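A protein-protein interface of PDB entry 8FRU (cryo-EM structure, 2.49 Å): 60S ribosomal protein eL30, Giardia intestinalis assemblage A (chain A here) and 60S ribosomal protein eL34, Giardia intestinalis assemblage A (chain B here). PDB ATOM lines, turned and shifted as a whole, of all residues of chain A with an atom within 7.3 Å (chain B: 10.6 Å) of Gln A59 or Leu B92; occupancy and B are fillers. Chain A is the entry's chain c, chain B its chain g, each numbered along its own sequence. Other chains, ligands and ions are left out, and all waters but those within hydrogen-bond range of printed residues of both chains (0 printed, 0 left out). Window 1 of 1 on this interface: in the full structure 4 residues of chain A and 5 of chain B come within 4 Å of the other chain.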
ATOM      1  N   THR A  31     -11.805 -32.051  19.008  1.00  0.00           N
ATOM      2  CA  THR A  31     -12.724 -31.297  19.846  1.00  0.00           C
ATOM      3  C   THR A  31     -13.485 -32.172  20.831  1.00  0.00           C
ATOM      4  O   THR A  31     -13.710 -31.756  21.973  1.00  0.00           O
ATOM      5  CB  THR A  31     -13.716 -30.534  18.966  1.00  0.00           C
ATOM      6  OG1 THR A  31     -13.012 -29.551  18.199  1.00  0.00           O
ATOM      7  CG2 THR A  31     -14.756 -29.839  19.821  1.00  0.00           C
ATOM      8  N   ILE A  35     -13.379 -31.775  24.916  1.00  0.00           N
ATOM      9  CA  ILE A  35     -14.507 -31.556  25.816  1.00  0.00           C
ATOM     10  C   ILE A  35     -14.564 -32.624  26.896  1.00  0.00           C
ATOM     11  O   ILE A  35     -14.797 -32.316  28.074  1.00  0.00           O
ATOM     12  CB  ILE A  35     -15.827 -31.491  25.029  1.00  0.00           C
ATOM     13  CG1 ILE A  35     -15.820 -30.297  24.081  1.00  0.00           C
ATOM     14  CG2 ILE A  35     -17.000 -31.417  25.970  1.00  0.00           C
ATOM     15  CD1 ILE A  35     -17.185 -29.939  23.547  1.00  0.00           C
ATOM     16  N   ILE A  38     -11.777 -31.690  29.481  1.00  0.00           N
ATOM     17  CA  ILE A  38     -12.009 -30.487  30.280  1.00  0.00           C
ATOM     18  C   ILE A  38     -13.135 -30.707  31.280  1.00  0.00           C
ATOM     19  O   ILE A  38     -13.057 -30.256  32.428  1.00  0.00           O
ATOM     20  CB  ILE A  38     -12.284 -29.269  29.380  1.00  0.00           C
ATOM     21  CG1 ILE A  38     -11.436 -29.326  28.116  1.00  0.00           C
ATOM     22  CG2 ILE A  38     -12.007 -27.990  30.122  1.00  0.00           C
ATOM     23  CD1 ILE A  38     -11.973 -28.480  26.978  1.00  0.00           C
ATOM     24  N   PRO A  53     -14.624 -22.811  14.528  1.00  0.00           N
ATOM     25  CA  PRO A  53     -15.989 -22.291  14.389  1.00  0.00           C
ATOM     26  C   PRO A  53     -16.430 -21.554  15.642  1.00  0.00           C
ATOM     27  O   PRO A  53     -16.139 -21.986  16.766  1.00  0.00           O
ATOM     28  CB  PRO A  53     -16.828 -23.554  14.150  1.00  0.00           C
ATOM     29  CG  PRO A  53     -15.977 -24.676  14.619  1.00  0.00           C
ATOM     30  CD  PRO A  53     -14.570 -24.273  14.392  1.00  0.00           C
ATOM     31  N   PRO A  54     -17.161 -20.446  15.487  1.00  0.00           N
ATOM     32  CA  PRO A  54     -17.444 -19.579  16.646  1.00  0.00           C
ATOM     33  C   PRO A  54     -18.224 -20.236  17.774  1.00  0.00           C
ATOM     34  O   PRO A  54     -17.949 -19.954  18.948  1.00  0.00           O
ATOM     35  CB  PRO A  54     -18.232 -18.426  16.009  1.00  0.00           C
ATOM     36  CG  PRO A  54     -18.840 -19.033  14.779  1.00  0.00           C
ATOM     37  CD  PRO A  54     -17.761 -19.919  14.253  1.00  0.00           C
ATOM     38  N   LEU A  55     -19.194 -21.101  17.465  1.00  0.00           N
ATOM     39  CA  LEU A  55     -19.995 -21.687  18.535  1.00  0.00           C
ATOM     40  C   LEU A  55     -19.186 -22.684  19.353  1.00  0.00           C
ATOM     41  O   LEU A  55     -19.326 -22.736  20.581  1.00  0.00           O
ATOM     42  CB  LEU A  55     -21.244 -22.344  17.950  1.00  0.00           C
ATOM     43  CG  LEU A  55     -22.154 -23.113  18.910  1.00  0.00           C
ATOM     44  CD1 LEU A  55     -22.637 -22.198  20.019  1.00  0.00           C
ATOM     45  CD2 LEU A  55     -23.335 -23.727  18.179  1.00  0.00           C
ATOM     46  N   VAL A  56     -18.306 -23.449  18.704  1.00  0.00           N
ATOM     47  CA  VAL A  56     -17.400 -24.306  19.458  1.00  0.00           C
ATOM     48  C   VAL A  56     -16.454 -23.456  20.290  1.00  0.00           C
ATOM     49  O   VAL A  56     -16.110 -23.819  21.420  1.00  0.00           O
ATOM     50  CB  VAL A  56     -16.624 -25.246  18.516  1.00  0.00           C
ATOM     51  CG1 VAL A  56     -15.741 -26.175  19.317  1.00  0.00           C
ATOM     52  CG2 VAL A  56     -17.573 -26.047  17.644  1.00  0.00           C
ATOM     53  N   LYS A  57     -16.038 -22.305  19.761  1.00  0.00           N
ATOM     54  CA  LYS A  57     -15.196 -21.401  20.530  1.00  0.00           C
ATOM     55  C   LYS A  57     -15.890 -20.971  21.809  1.00  0.00           C
ATOM     56  O   LYS A  57     -15.304 -21.033  22.897  1.00  0.00           O
ATOM     57  CB  LYS A  57     -14.849 -20.178  19.688  1.00  0.00           C
ATOM     58  CG  LYS A  57     -13.485 -20.217  19.055  1.00  0.00           C
ATOM     59  CD  LYS A  57     -12.968 -18.814  18.805  1.00  0.00           C
ATOM     60  CE  LYS A  57     -12.761 -18.053  20.099  1.00  0.00           C
ATOM     61  NZ  LYS A  57     -11.574 -18.541  20.844  1.00  0.00           N
ATOM     62  N   SER A  58     -17.151 -20.555  21.699  1.00  0.00           N
ATOM     63  CA  SER A  58     -17.895 -20.121  22.874  1.00  0.00           C
ATOM     64  C   SER A  58     -18.049 -21.260  23.870  1.00  0.00           C
ATOM     65  O   SER A  58     -17.823 -21.083  25.073  1.00  0.00           O
ATOM     66  CB  SER A  58     -19.264 -19.591  22.462  1.00  0.00           C
ATOM     67  OG  SER A  58     -19.195 -18.924  21.217  1.00  0.00           O
ATOM     68  N   GLN A  59     -18.427 -22.441  23.385  1.00  0.00           N
ATOM     69  CA  GLN A  59     -18.659 -23.558  24.291  1.00  0.00           C
ATOM     70  C   GLN A  59     -17.389 -23.923  25.046  1.00  0.00           C
ATOM     71  O   GLN A  59     -17.407 -24.102  26.271  1.00  0.00           O
ATOM     72  CB  GLN A  59     -19.182 -24.756  23.507  1.00  0.00           C
ATOM     73  CG  GLN A  59     -19.683 -25.882  24.373  1.00  0.00           C
ATOM     74  CD  GLN A  59     -20.017 -27.108  23.567  1.00  0.00           C
ATOM     75  OE1 GLN A  59     -19.752 -27.161  22.369  1.00  0.00           O
ATOM     76  NE2 GLN A  59     -20.607 -28.101  24.214  1.00  0.00           N
ATOM     77  N   VAL A  60     -16.267 -24.025  24.334  1.00  0.00           N
ATOM     78  CA  VAL A  60     -15.023 -24.421  24.981  1.00  0.00           C
ATOM     79  C   VAL A  60     -14.560 -23.342  25.952  1.00  0.00           C
ATOM     80  O   VAL A  60     -14.101 -23.647  27.058  1.00  0.00           O
ATOM     81  CB  VAL A  60     -13.951 -24.746  23.926  1.00  0.00           C
ATOM     82  CG1 VAL A  60     -12.604 -24.971  24.581  1.00  0.00           C
ATOM     83  CG2 VAL A  60     -14.357 -25.964  23.129  1.00  0.00           C
ATOM     84  N   ASP A  61     -14.680 -22.069  25.570  1.00  0.00           N
ATOM     85  CA  ASP A  61     -14.342 -20.988  26.486  1.00  0.00           C
ATOM     86  C   ASP A  61     -15.132 -21.103  27.783  1.00  0.00           C
ATOM     87  O   ASP A  61     -14.567 -21.052  28.882  1.00  0.00           O
ATOM     88  CB  ASP A  61     -14.608 -19.638  25.824  1.00  0.00           C
ATOM     89  CG  ASP A  61     -13.360 -19.018  25.244  1.00  0.00           C
ATOM     90  OD1 ASP A  61     -12.304 -19.681  25.275  1.00  0.00           O
ATOM     91  OD2 ASP A  61     -13.431 -17.868  24.764  1.00  0.00           O
ATOM     92  N   TYR A  62     -16.453 -21.232  27.667  1.00  0.00           N
ATOM     93  CA  TYR A  62     -17.307 -21.234  28.847  1.00  0.00           C
ATOM     94  C   TYR A  62     -17.010 -22.436  29.737  1.00  0.00           C
ATOM     95  O   TYR A  62     -16.984 -22.318  30.968  1.00  0.00           O
ATOM     96  CB  TYR A  62     -18.771 -21.207  28.409  1.00  0.00           C
ATOM     97  CG  TYR A  62     -19.794 -21.345  29.508  1.00  0.00           C
ATOM     98  CD1 TYR A  62     -20.254 -22.584  29.910  1.00  0.00           C
ATOM     99  CD2 TYR A  62     -20.344 -20.223  30.105  1.00  0.00           C
ATOM    100  CE1 TYR A  62     -21.197 -22.704  30.897  1.00  0.00           C
ATOM    101  CE2 TYR A  62     -21.293 -20.335  31.092  1.00  0.00           C
ATOM    102  CZ  TYR A  62     -21.717 -21.577  31.482  1.00  0.00           C
ATOM    103  OH  TYR A  62     -22.663 -21.695  32.468  1.00  0.00           O
ATOM    104  N   LEU A  63     -16.761 -23.600  29.137  1.00  0.00           N
ATOM    105  CA  LEU A  63     -16.422 -24.767  29.949  1.00  0.00           C
ATOM    106  C   LEU A  63     -15.086 -24.581  30.656  1.00  0.00           C
ATOM    107  O   LEU A  63     -14.948 -24.923  31.839  1.00  0.00           O
ATOM    108  CB  LEU A  63     -16.391 -26.023  29.083  1.00  0.00           C
ATOM    109  CG  LEU A  63     -17.739 -26.575  28.621  1.00  0.00           C
ATOM    110  CD1 LEU A  63     -17.523 -27.767  27.709  1.00  0.00           C
ATOM    111  CD2 LEU A  63     -18.613 -26.945  29.802  1.00  0.00           C
ATOM    112  N   CYS A  64     -14.091 -24.034  29.955  1.00  0.00           N
ATOM    113  CA  CYS A  64     -12.809 -23.768  30.593  1.00  0.00           C
ATOM    114  C   CYS A  64     -12.984 -22.824  31.772  1.00  0.00           C
ATOM    115  O   CYS A  64     -12.363 -23.006  32.824  1.00  0.00           O
ATOM    116  CB  CYS A  64     -11.827 -23.187  29.578  1.00  0.00           C
ATOM    117  SG  CYS A  64     -11.210 -24.366  28.362  1.00  0.00           S
ATOM    118  N   HIS A  65     -13.834 -21.810  31.612  1.00  0.00           N
ATOM    119  CA  HIS A  65     -14.152 -20.933  32.730  1.00  0.00           C
ATOM    120  C   HIS A  65     -14.760 -21.710  33.887  1.00  0.00           C
ATOM    121  O   HIS A  65     -14.402 -21.490  35.047  1.00  0.00           O
ATOM    122  CB  HIS A  65     -15.108 -19.833  32.284  1.00  0.00           C
ATOM    123  CG  HIS A  65     -15.513 -18.913  33.389  1.00  0.00           C
ATOM    124  ND1 HIS A  65     -16.830 -18.634  33.681  1.00  0.00           N
ATOM    125  CD2 HIS A  65     -14.774 -18.218  34.284  1.00  0.00           C
ATOM    126  CE1 HIS A  65     -16.885 -17.801  34.704  1.00  0.00           C
ATOM    127  NE2 HIS A  65     -15.650 -17.533  35.089  1.00  0.00           N
ATOM    128  N   ARG B  84     -29.457 -28.774  18.319  1.00  0.00           N
ATOM    129  CA  ARG B  84     -28.410 -28.544  19.309  1.00  0.00           C
ATOM    130  C   ARG B  84     -27.794 -27.163  19.149  1.00  0.00           C
ATOM    131  O   ARG B  84     -27.569 -26.459  20.138  1.00  0.00           O
ATOM    132  CB  ARG B  84     -27.329 -29.612  19.193  1.00  0.00           C
ATOM    133  CG  ARG B  84     -27.555 -30.821  20.061  1.00  0.00           C
ATOM    134  CD  ARG B  84     -26.297 -31.658  20.132  1.00  0.00           C
ATOM    135  NE  ARG B  84     -25.104 -30.842  19.954  1.00  0.00           N
ATOM    136  CZ  ARG B  84     -24.046 -30.877  20.750  1.00  0.00           C
ATOM    137  NH1 ARG B  84     -24.002 -31.672  21.805  1.00  0.00           N
ATOM    138  NH2 ARG B  84     -23.005 -30.096  20.482  1.00  0.00           N
ATOM    139  N   ALA B  85     -27.512 -26.760  17.912  1.00  0.00           N
ATOM    140  CA  ALA B  85     -26.876 -25.469  17.687  1.00  0.00           C
ATOM    141  C   ALA B  85     -27.750 -24.327  18.187  1.00  0.00           C
ATOM    142  O   ALA B  85     -27.252 -23.370  18.788  1.00  0.00           O
ATOM    143  CB  ALA B  85     -26.562 -25.298  16.204  1.00  0.00           C
ATOM    144  N   HIS B  86     -29.053 -24.406  17.941  1.00  0.00           N
ATOM    145  CA  HIS B  86     -29.954 -23.363  18.408  1.00  0.00           C
ATOM    146  C   HIS B  86     -30.013 -23.317  19.929  1.00  0.00           C
ATOM    147  O   HIS B  86     -30.061 -22.234  20.519  1.00  0.00           O
ATOM    148  CB  HIS B  86     -31.342 -23.581  17.820  1.00  0.00           C
ATOM    149  CG  HIS B  86     -31.473 -23.113  16.406  1.00  0.00           C
ATOM    150  ND1 HIS B  86     -31.058 -23.868  15.332  1.00  0.00           N
ATOM    151  CD2 HIS B  86     -31.978 -21.970  15.888  1.00  0.00           C
ATOM    152  CE1 HIS B  86     -31.297 -23.208  14.215  1.00  0.00           C
ATOM    153  NE2 HIS B  86     -31.856 -22.054  14.525  1.00  0.00           N
ATOM    154  N   ILE B  87     -30.024 -24.479  20.580  1.00  0.00           N
ATOM    155  CA  ILE B  87     -30.038 -24.509  22.038  1.00  0.00           C
ATOM    156  C   ILE B  87     -28.730 -23.961  22.592  1.00  0.00           C
ATOM    157  O   ILE B  87     -28.725 -23.114  23.491  1.00  0.00           O
ATOM    158  CB  ILE B  87     -30.313 -25.936  22.543  1.00  0.00           C
ATOM    159  CG1 ILE B  87     -31.746 -26.350  22.222  1.00  0.00           C
ATOM    160  CG2 ILE B  87     -30.073 -26.032  24.030  1.00  0.00           C
ATOM    161  CD1 ILE B  87     -31.989 -27.823  22.351  1.00  0.00           C
ATOM    162  N   LEU B  88     -27.601 -24.428  22.060  1.00  0.00           N
ATOM    163  CA  LEU B  88     -26.311 -23.925  22.516  1.00  0.00           C
ATOM    164  C   LEU B  88     -26.171 -22.438  22.238  1.00  0.00           C
ATOM    165  O   LEU B  88     -25.697 -21.680  23.090  1.00  0.00           O
ATOM    166  CB  LEU B  88     -25.178 -24.689  21.839  1.00  0.00           C
ATOM    167  CG  LEU B  88     -24.898 -26.106  22.323  1.00  0.00           C
ATOM    168  CD1 LEU B  88     -23.802 -26.718  21.488  1.00  0.00           C
ATOM    169  CD2 LEU B  88     -24.512 -26.095  23.776  1.00  0.00           C
ATOM    170  N   GLU B  89     -26.572 -22.002  21.048  1.00  0.00           N
ATOM    171  CA  GLU B  89     -26.408 -20.601  20.682  1.00  0.00           C
ATOM    172  C   GLU B  89     -27.260 -19.691  21.556  1.00  0.00           C
ATOM    173  O   GLU B  89     -26.802 -18.626  21.979  1.00  0.00           O
ATOM    174  CB  GLU B  89     -26.750 -20.409  19.207  1.00  0.00           C
ATOM    175  CG  GLU B  89     -26.065 -19.231  18.562  1.00  0.00           C
ATOM    176  CD  GLU B  89     -27.028 -18.376  17.773  1.00  0.00           C
ATOM    177  OE1 GLU B  89     -28.221 -18.737  17.713  1.00  0.00           O
ATOM    178  OE2 GLU B  89     -26.599 -17.341  17.220  1.00  0.00           O
ATOM    179  N   SER B  90     -28.506 -20.081  21.827  1.00  0.00           N
ATOM    180  CA  SER B  90     -29.370 -19.242  22.650  1.00  0.00           C
ATOM    181  C   SER B  90     -28.873 -19.172  24.085  1.00  0.00           C
ATOM    182  O   SER B  90     -28.883 -18.100  24.697  1.00  0.00           O
ATOM    183  CB  SER B  90     -30.807 -19.759  22.607  1.00  0.00           C
ATOM    184  OG  SER B  90     -30.992 -20.828  23.514  1.00  0.00           O
ATOM    185  N   PHE B  91     -28.446 -20.301  24.646  1.00  0.00           N
ATOM    186  CA  PHE B  91     -27.978 -20.294  26.025  1.00  0.00           C
ATOM    187  C   PHE B  91     -26.695 -19.487  26.171  1.00  0.00           C
ATOM    188  O   PHE B  91     -26.602 -18.604  27.028  1.00  0.00           O
ATOM    189  CB  PHE B  91     -27.766 -21.721  26.516  1.00  0.00           C
ATOM    190  CG  PHE B  91     -26.909 -21.809  27.734  1.00  0.00           C
ATOM    191  CD1 PHE B  91     -27.334 -21.270  28.933  1.00  0.00           C
ATOM    192  CD2 PHE B  91     -25.665 -22.407  27.679  1.00  0.00           C
ATOM    193  CE1 PHE B  91     -26.542 -21.345  30.053  1.00  0.00           C
ATOM    194  CE2 PHE B  91     -24.871 -22.480  28.797  1.00  0.00           C
ATOM    195  CZ  PHE B  91     -25.311 -21.949  29.985  1.00  0.00           C
ATOM    196  N   LEU B  92     -25.694 -19.772  25.336  1.00  0.00           N
ATOM    197  CA  LEU B  92     -24.423 -19.068  25.453  1.00  0.00           C
ATOM    198  C   LEU B  92     -24.584 -17.580  25.185  1.00  0.00           C
ATOM    199  O   LEU B  92     -23.850 -16.767  25.752  1.00  0.00           O
ATOM    200  CB  LEU B  92     -23.392 -19.666  24.498  1.00  0.00           C
ATOM    201  CG  LEU B  92     -22.905 -21.085  24.790  1.00  0.00           C
ATOM    202  CD1 LEU B  92     -22.349 -21.712  23.538  1.00  0.00           C
ATOM    203  CD2 LEU B  92     -21.864 -21.091  25.894  1.00  0.00           C
ATOM    204  N   ASN B  93     -25.517 -17.204  24.316  1.00  0.00           N
ATOM    205  CA  ASN B  93     -25.713 -15.790  24.027  1.00  0.00           C
ATOM    206  C   ASN B  93     -26.427 -15.087  25.170  1.00  0.00           C
ATOM    207  O   ASN B  93     -26.051 -13.974  25.552  1.00  0.00           O
ATOM    208  CB  ASN B  93     -26.497 -15.626  22.728  1.00  0.00           C
ATOM    209  CG  ASN B  93     -25.616 -15.227  21.567  1.00  0.00           C
ATOM    210  OD1 ASN B  93     -24.823 -14.292  21.667  1.00  0.00           O
ATOM    211  ND2 ASN B  93     -25.748 -15.936  20.455  1.00  0.00           N
ATOM    212  N   GLU B  94     -27.462 -15.716  25.725  1.00  0.00           N
ATOM    213  CA  GLU B  94     -28.230 -15.086  26.787  1.00  0.00           C
ATOM    214  C   GLU B  94     -27.468 -15.073  28.100  1.00  0.00           C
ATOM    215  O   GLU B  94     -27.790 -14.276  28.983  1.00  0.00           O
ATOM    216  CB  GLU B  94     -29.572 -15.797  26.951  1.00  0.00           C
ATOM    217  CG  GLU B  94     -30.646 -14.965  27.635  1.00  0.00           C
ATOM    218  CD  GLU B  94     -31.031 -15.492  29.001  1.00  0.00           C
ATOM    219  OE1 GLU B  94     -31.342 -16.697  29.114  1.00  0.00           O
ATOM    220  OE2 GLU B  94     -31.033 -14.693  29.961  1.00  0.00           O
ATOM    221  N   GLU B  95     -26.470 -15.943  28.249  1.00  0.00           N
ATOM    222  CA  GLU B  95     -25.623 -15.903  29.433  1.00  0.00           C
ATOM    223  C   GLU B  95     -24.664 -14.716  29.386  1.00  0.00           C
ATOM    224  O   GLU B  95     -24.497 -14.000  30.379  1.00  0.00           O
ATOM    225  CB  GLU B  95     -24.863 -17.221  29.568  1.00  0.00           C
ATOM    226  CG  GLU B  95     -23.962 -17.301  30.772  1.00  0.00           C
ATOM    227  CD  GLU B  95     -22.574 -16.780  30.481  1.00  0.00           C
ATOM    228  OE1 GLU B  95     -21.858 -17.430  29.689  1.00  0.00           O
ATOM    229  OE2 GLU B  95     -22.200 -15.724  31.033  1.00  0.00           O
ATOM    230  N   ASN B  96     -24.026 -14.489  28.237  1.00  0.00           N
ATOM    231  CA  ASN B  96     -23.146 -13.332  28.113  1.00  0.00           C
ATOM    232  C   ASN B  96     -23.940 -12.040  27.981  1.00  0.00           C
ATOM    233  O   ASN B  96     -23.599 -11.028  28.603  1.00  0.00           O
ATOM    234  CB  ASN B  96     -22.209 -13.505  26.920  1.00  0.00           C
ATOM    235  CG  ASN B  96     -21.317 -14.722  27.049  1.00  0.00           C
ATOM    236  OD1 ASN B  96     -20.709 -14.953  28.092  1.00  0.00           O
ATOM    237  ND2 ASN B  96     -21.225 -15.502  25.983  1.00  0.00           N
ATOM    238  N   GLN B  97     -25.004 -12.056  27.188  1.00  0.00           N
ATOM    239  CA  GLN B  97     -25.748 -10.842  26.875  1.00  0.00           C
ATOM    240  C   GLN B  97     -26.362 -10.230  28.126  1.00  0.00           C
ATOM    241  O   GLN B  97     -25.733  -9.412  28.797  1.00  0.00           O
ATOM    242  CB  GLN B  97     -26.831 -11.139  25.840  1.00  0.00           C
ATOM    243  CG  GLN B  97     -26.309 -11.206  24.410  1.00  0.00           C
ATOM    244  CD  GLN B  97     -27.281 -11.876  23.459  1.00  0.00           C
ATOM    245  OE1 GLN B  97     -26.911 -12.780  22.712  1.00  0.00           O
ATOM    246  NE2 GLN B  97     -28.529 -11.428  23.473  1.00  0.00           N
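Leu A55 touches Ala B85.
Leu A55 touches Leu B88.
Leu A55 touches Leu B92.
CD1 of Leu B92 touches CB of Ser A58 (3.9 Å).
N of Gln A59 touches CD1 of Leu B92, 3.99 Å away.
OH of Tyr A62 touches CZ of Phe B91 (3.6 Å).
CB of Tyr A62 touches CD2 of Leu B92 (3.99 Å).
CD2 of Tyr A62 touches OE1 of Glu B95 (3.2 Å).
Of the 16 printed residues of chain A, 4 touch a printed residue of chain B.
Of the 14 printed residues of chain B, 5 touch a printed residue of chain A.
Hydrophobic or aromatic side chains of chain B that line the printed part of chain A: Leu B88, Phe B91 and Leu B92.
Among the printed residues, 8 pairs touch across the chains.
Among the printed residues, no Asp or Glu carboxylate lies within 4 Å of a Lys or Arg side-chain nitrogen of the other chain.
Of the printed residues of chain B, Gln A59 touches Leu B92.
Printed residues of chain A within 4 Å of Leu B92: Leu A55, Ser A58, Gln A59 and Tyr A62.
Ser A58 touches one residue of chain B.
Printed residues of chain B within 4 Å of Leu A55: Ala B85 (3.98 Å), Leu B88 (3.997 Å) and Leu B92 (3.6 Å).
Of the printed residues of chain A, Glu B95 touches Tyr A62 (3.2 Å).
Of the printed residues of chain A, Ala B85 touches Leu A55 (3.98 Å).
The nearest printed residue of chain B that does not touch Gln A59 is Leu B88 (4.2 Å).
The nearest printed residue of chain A that does not touch Leu B92 is Val A60 (6.5 Å).
The side-chain hydroxyl (OG) of Ser A58 lies within hydrogen-bond range of the backbone carbonyl oxygen (O) of Pro A54, 2.8 Å away.
O of Leu B92 sits at hydrogen-bond distance from ND2 of Asn B96, 2.9 Å away.
The side-chain carboxylate of Glu B95 lies close to the side-chain amide oxygen of Asn B96 (3.2 Å).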
